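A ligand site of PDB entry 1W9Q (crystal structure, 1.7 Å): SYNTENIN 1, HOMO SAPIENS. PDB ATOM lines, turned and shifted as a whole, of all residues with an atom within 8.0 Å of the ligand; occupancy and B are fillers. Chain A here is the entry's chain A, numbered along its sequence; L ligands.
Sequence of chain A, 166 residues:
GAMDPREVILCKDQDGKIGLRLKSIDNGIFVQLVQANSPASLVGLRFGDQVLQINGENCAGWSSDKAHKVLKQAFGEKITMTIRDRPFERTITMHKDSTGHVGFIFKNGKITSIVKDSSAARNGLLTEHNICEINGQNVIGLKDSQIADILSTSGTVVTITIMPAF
An oxygen (O2) of the ligand lies within salt-bridge range of the guanidinium group (NH2) of Arg 122 (2.8 Å). The side-chain amide nitrogen (ND2) of Asn 123 lies within hydrogen-bond range of an oxygen (O1) of the ligand, at 3.0 Å. OG of Ser 119 lies within hydrogen-bond range of O2 of the ligand (2.6 Å).
The backbone carbonyl oxygen of Asp 117 is in hydrogen-bond range of the guanidinium group of Arg 122, at 3.3 Å. O of Thr 93 sits close to OD1 of Asn 123, 3.1 Å away. N of Ser 119 sits at hydrogen-bond distance from O of Val 102. O of Ser 119 is in hydrogen-bond range of ND2 of Asn 123, at 2.9 Å. OG of Ser 119 is in hydrogen-bond range of N of His 95 (2.9 Å).
His 95 touches the ligand. Hydrophobic or aromatic side chains within 4 Å of the ligand: His 95. Within 4 Å of the ligand: His 95, Ser 119, Arg 122 and Asn 123. Along chain A the residues within 4 Å of the ligand span positions 95 to 123. The nearest printed residue that does not touch the ligand is Thr 93 (4.1 Å).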
ATOM      1  N   ILE A  92       0.416  18.668  37.690  1.00  0.00           N
ATOM      2  CA  ILE A  92       0.695  17.951  36.442  1.00  0.00           C
ATOM      3  C   ILE A  92       2.162  18.116  36.105  1.00  0.00           C
ATOM      4  O   ILE A  92       2.683  19.231  36.090  1.00  0.00           O
ATOM      5  CB  ILE A  92      -0.176  18.492  35.275  1.00  0.00           C
ATOM      6  CG1 ILE A  92      -1.661  18.355  35.595  1.00  0.00           C
ATOM      7  CG2 ILE A  92       0.179  17.768  33.938  1.00  0.00           C
ATOM      8  CD1 ILE A  92      -2.336  17.171  34.985  1.00  0.00           C
ATOM      9  N   THR A  93       2.821  17.001  35.771  1.00  0.00           N
ATOM     10  CA  THR A  93       4.209  17.034  35.397  1.00  0.00           C
ATOM     11  C   THR A  93       4.333  16.705  33.922  1.00  0.00           C
ATOM     12  O   THR A  93       3.785  15.704  33.449  1.00  0.00           O
ATOM     13  CB  THR A  93       5.018  16.046  36.235  1.00  0.00           C
ATOM     14  OG1 THR A  93       5.003  16.455  37.622  1.00  0.00           O
ATOM     15  CG2 THR A  93       6.495  16.137  35.846  1.00  0.00           C
ATOM     16  N   MET A  94       5.025  17.564  33.195  1.00  0.00           N
ATOM     17  CA  MET A  94       5.228  17.366  31.759  1.00  0.00           C
ATOM     18  C   MET A  94       6.710  17.357  31.439  1.00  0.00           C
ATOM     19  O   MET A  94       7.527  17.737  32.283  1.00  0.00           O
ATOM     20  CB  MET A  94       4.512  18.443  30.949  1.00  0.00           C
ATOM     21  CG  MET A  94       2.984  18.288  30.921  1.00  0.00           C
ATOM     22  SD  MET A  94       2.208  19.913  30.723  1.00  0.00           S
ATOM     23  CE  MET A  94       2.605  20.671  32.259  1.00  0.00           C
ATOM     24  N   HIS A  95       7.058  16.878  30.234  1.00  0.00           N
ATOM     25  CA  HIS A  95       8.445  16.838  29.765  1.00  0.00           C
ATOM     26  C   HIS A  95       8.486  17.640  28.463  1.00  0.00           C
ATOM     27  O   HIS A  95       7.667  17.419  27.568  1.00  0.00           O
ATOM     28  CB  HIS A  95       8.875  15.403  29.443  1.00  0.00           C
ATOM     29  CG  HIS A  95       9.262  14.575  30.633  1.00  0.00           C
ATOM     30  ND1 HIS A  95       8.592  14.602  31.831  1.00  0.00           N
ATOM     31  CD2 HIS A  95      10.250  13.658  30.782  1.00  0.00           C
ATOM     32  CE1 HIS A  95       9.160  13.768  32.681  1.00  0.00           C
ATOM     33  NE2 HIS A  95      10.178  13.190  32.071  1.00  0.00           N
ATOM     34  N   LYS A  96       9.422  18.575  28.339  1.00  0.00           N
ATOM     35  CA  LYS A  96       9.605  19.288  27.063  1.00  0.00           C
ATOM     36  C   LYS A  96       9.941  18.311  25.944  1.00  0.00           C
ATOM     37  O   LYS A  96      10.660  17.330  26.175  1.00  0.00           O
ATOM     38  CB  LYS A  96      10.750  20.308  27.200  1.00  0.00           C
ATOM     39  CG  LYS A  96      10.414  21.518  28.068  1.00  0.00           C
ATOM     40  CD  LYS A  96      11.576  22.516  28.096  1.00  0.00           C
ATOM     41  CE  LYS A  96      11.157  23.776  28.823  1.00  0.00           C
ATOM     42  NZ  LYS A  96      12.238  24.840  28.774  1.00  0.00           N
ATOM     43  N   ASP A  97       9.458  18.588  24.737  1.00  0.00           N
ATOM     44  CA  ASP A  97       9.801  17.720  23.592  1.00  0.00           C
ATOM     45  C   ASP A  97      11.206  18.044  23.072  1.00  0.00           C
ATOM     46  O   ASP A  97      11.933  18.819  23.682  1.00  0.00           O
ATOM     47  CB  ASP A  97       8.729  17.758  22.480  1.00  0.00           C
ATOM     48  CG  ASP A  97       8.585  19.125  21.788  1.00  0.00           C
ATOM     49  OD1 ASP A  97       9.465  19.997  21.907  1.00  0.00           O
ATOM     50  OD2 ASP A  97       7.581  19.401  21.095  1.00  0.00           O
ATOM     51  N   VAL A 102       6.387  21.973  25.975  1.00  0.00           N
ATOM     52  CA  VAL A 102       5.592  21.014  26.781  1.00  0.00           C
ATOM     53  C   VAL A 102       4.203  20.794  26.202  1.00  0.00           C
ATOM     54  O   VAL A 102       3.586  19.747  26.429  1.00  0.00           O
ATOM     55  CB  VAL A 102       5.476  21.404  28.259  1.00  0.00           C
ATOM     56  CG1 VAL A 102       6.801  21.148  28.971  1.00  0.00           C
ATOM     57  CG2 VAL A 102       5.003  22.842  28.418  1.00  0.00           C
ATOM     58  N   ASP A 117      -0.842  15.832  20.723  1.00  0.00           N
ATOM     59  CA  ASP A 117       0.147  14.803  20.998  1.00  0.00           C
ATOM     60  C   ASP A 117       1.418  15.260  21.716  1.00  0.00           C
ATOM     61  O   ASP A 117       2.477  14.630  21.630  1.00  0.00           O
ATOM     62  CB  ASP A 117       0.463  14.054  19.719  1.00  0.00           C
ATOM     63  CG  ASP A 117      -0.738  13.310  19.198  1.00  0.00           C
ATOM     64  OD1 ASP A 117      -1.643  12.949  20.013  1.00  0.00           O
ATOM     65  OD2 ASP A 117      -0.851  13.035  17.993  1.00  0.00           O
ATOM     66  N   SER A 118       1.288  16.353  22.438  1.00  0.00           N
ATOM     67  CA  SER A 118       2.361  16.891  23.262  1.00  0.00           C
ATOM     68  C   SER A 118       2.380  16.173  24.596  1.00  0.00           C
ATOM     69  O   SER A 118       1.462  15.391  24.914  1.00  0.00           O
ATOM     70  CB  SER A 118       2.090  18.386  23.487  1.00  0.00           C
ATOM     71  OG  SER A 118       0.878  18.546  24.234  1.00  0.00           O
ATOM     72  N   SER A 119       3.395  16.452  25.421  1.00  0.00           N
ATOM     73  CA  SER A 119       3.381  15.983  26.797  1.00  0.00           C
ATOM     74  C   SER A 119       2.137  16.468  27.575  1.00  0.00           C
ATOM     75  O   SER A 119       1.568  15.722  28.381  1.00  0.00           O
ATOM     76  CB  SER A 119       4.660  16.417  27.515  1.00  0.00           C
ATOM     77  OG  SER A 119       4.739  15.842  28.807  1.00  0.00           O
ATOM     78  N   ALA A 120       1.725  17.720  27.334  1.00  0.00           N
ATOM     79  CA  ALA A 120       0.529  18.261  28.000  1.00  0.00           C
ATOM     80  C   ALA A 120      -0.694  17.431  27.603  1.00  0.00           C
ATOM     81  O   ALA A 120      -1.510  17.091  28.472  1.00  0.00           O
ATOM     82  CB  ALA A 120       0.320  19.722  27.655  1.00  0.00           C
ATOM     83  N   ALA A 121      -0.808  17.078  26.325  1.00  0.00           N
ATOM     84  CA  ALA A 121      -1.864  16.174  25.911  1.00  0.00           C
ATOM     85  C   ALA A 121      -1.799  14.824  26.602  1.00  0.00           C
ATOM     86  O   ALA A 121      -2.809  14.370  27.134  1.00  0.00           O
ATOM     87  CB  ALA A 121      -1.897  16.008  24.372  1.00  0.00           C
ATOM     88  N   ARG A 122      -0.618  14.193  26.594  1.00  0.00           N
ATOM     89  CA  ARG A 122      -0.474  12.868  27.193  1.00  0.00           C
ATOM     90  C   ARG A 122      -0.821  12.872  28.651  1.00  0.00           C
ATOM     91  O   ARG A 122      -1.369  11.890  29.181  1.00  0.00           O
ATOM     92  CB  ARG A 122       0.959  12.340  27.043  1.00  0.00           C
ATOM     93  CG  ARG A 122       1.280  11.938  25.607  1.00  0.00           C
ATOM     94  CD  ARG A 122       2.588  11.122  25.508  1.00  0.00           C
ATOM     95  NE  ARG A 122       3.737  11.914  25.966  1.00  0.00           N
ATOM     96  CZ  ARG A 122       4.425  12.763  25.191  1.00  0.00           C
ATOM     97  NH1 ARG A 122       4.062  12.953  23.928  1.00  0.00           N
ATOM     98  NH2 ARG A 122       5.477  13.410  25.685  1.00  0.00           N
ATOM     99  N   ASN A 123      -0.538  13.985  29.309  1.00  0.00           N
ATOM    100  CA  ASN A 123      -0.751  14.086  30.765  1.00  0.00           C
ATOM    101  C   ASN A 123      -2.150  14.601  31.128  1.00  0.00           C
ATOM    102  O   ASN A 123      -2.487  14.738  32.309  1.00  0.00           O
ATOM    103  CB  ASN A 123       0.357  14.932  31.391  1.00  0.00           C
ATOM    104  CG  ASN A 123       1.628  14.147  31.615  1.00  0.00           C
ATOM    105  OD1 ASN A 123       1.763  13.447  32.614  1.00  0.00           O
ATOM    106  ND2 ASN A 123       2.551  14.211  30.657  1.00  0.00           N
ATOM    107  N   THR A 156      14.000  20.157  31.189  1.00  0.00           N
ATOM    108  CA  THR A 156      13.060  19.256  30.506  1.00  0.00           C
ATOM    109  C   THR A 156      11.784  19.047  31.326  1.00  0.00           C
ATOM    110  O   THR A 156      10.688  19.213  30.796  1.00  0.00           O
ATOM    111  CB  THR A 156      13.737  17.922  30.242  1.00  0.00           C
ATOM    112  OG1 THR A 156      14.875  18.138  29.377  1.00  0.00           O
ATOM    113  CG2 THR A 156      12.830  16.987  29.436  1.00  0.00           C
ATOM    114  N   VAL A 157      11.932  18.741  32.614  1.00  0.00           N
ATOM    115  CA  VAL A 157      10.795  18.419  33.479  1.00  0.00           C
ATOM    116  C   VAL A 157      10.123  19.702  33.969  1.00  0.00           C
ATOM    117  O   VAL A 157      10.758  20.554  34.606  1.00  0.00           O
ATOM    118  CB  VAL A 157      11.188  17.505  34.673  1.00  0.00           C
ATOM    119  CG1 VAL A 157       9.996  17.308  35.643  1.00  0.00           C
ATOM    120  CG2 VAL A 157      11.731  16.144  34.189  1.00  0.00           C
ATOM    121  N   VAL A 158       8.836  19.850  33.660  1.00  0.00           N
ATOM    122  CA  VAL A 158       8.080  21.035  34.056  1.00  0.00           C
ATOM    123  C   VAL A 158       6.888  20.587  34.883  1.00  0.00           C
ATOM    124  O   VAL A 158       5.980  19.915  34.365  1.00  0.00           O
ATOM    125  CB  VAL A 158       7.616  21.839  32.814  1.00  0.00           C
ATOM    126  CG1 VAL A 158       6.724  23.033  33.212  1.00  0.00           C
ATOM    127  CG2 VAL A 158       8.838  22.309  31.955  1.00  0.00           C
HETATM  128  C1  LIG L   1       5.985  12.797  29.571  1.00  0.00           C
HETATM  129  O1  LIG L   1       5.241  12.980  30.752  1.00  0.00           O
HETATM  130  O2  LIG L   1       5.573  13.416  28.499  1.00  0.00           O
HETATM  131  C2  LIG L   1       7.213  11.953  29.538  1.00  0.00           C
HETATM  132  C3  LIG L   1       8.065  11.991  28.433  1.00  0.00           C
HETATM  133  C4  LIG L   1       9.226  11.199  28.417  1.00  0.00           C
HETATM  134  C5  LIG L   1       9.522  10.372  29.502  1.00  0.00           C
HETATM  135  C6  LIG L   1       8.668  10.324  30.606  1.00  0.00           C
HETATM  136  C7  LIG L   1       7.513  11.106  30.615  1.00  0.00           C
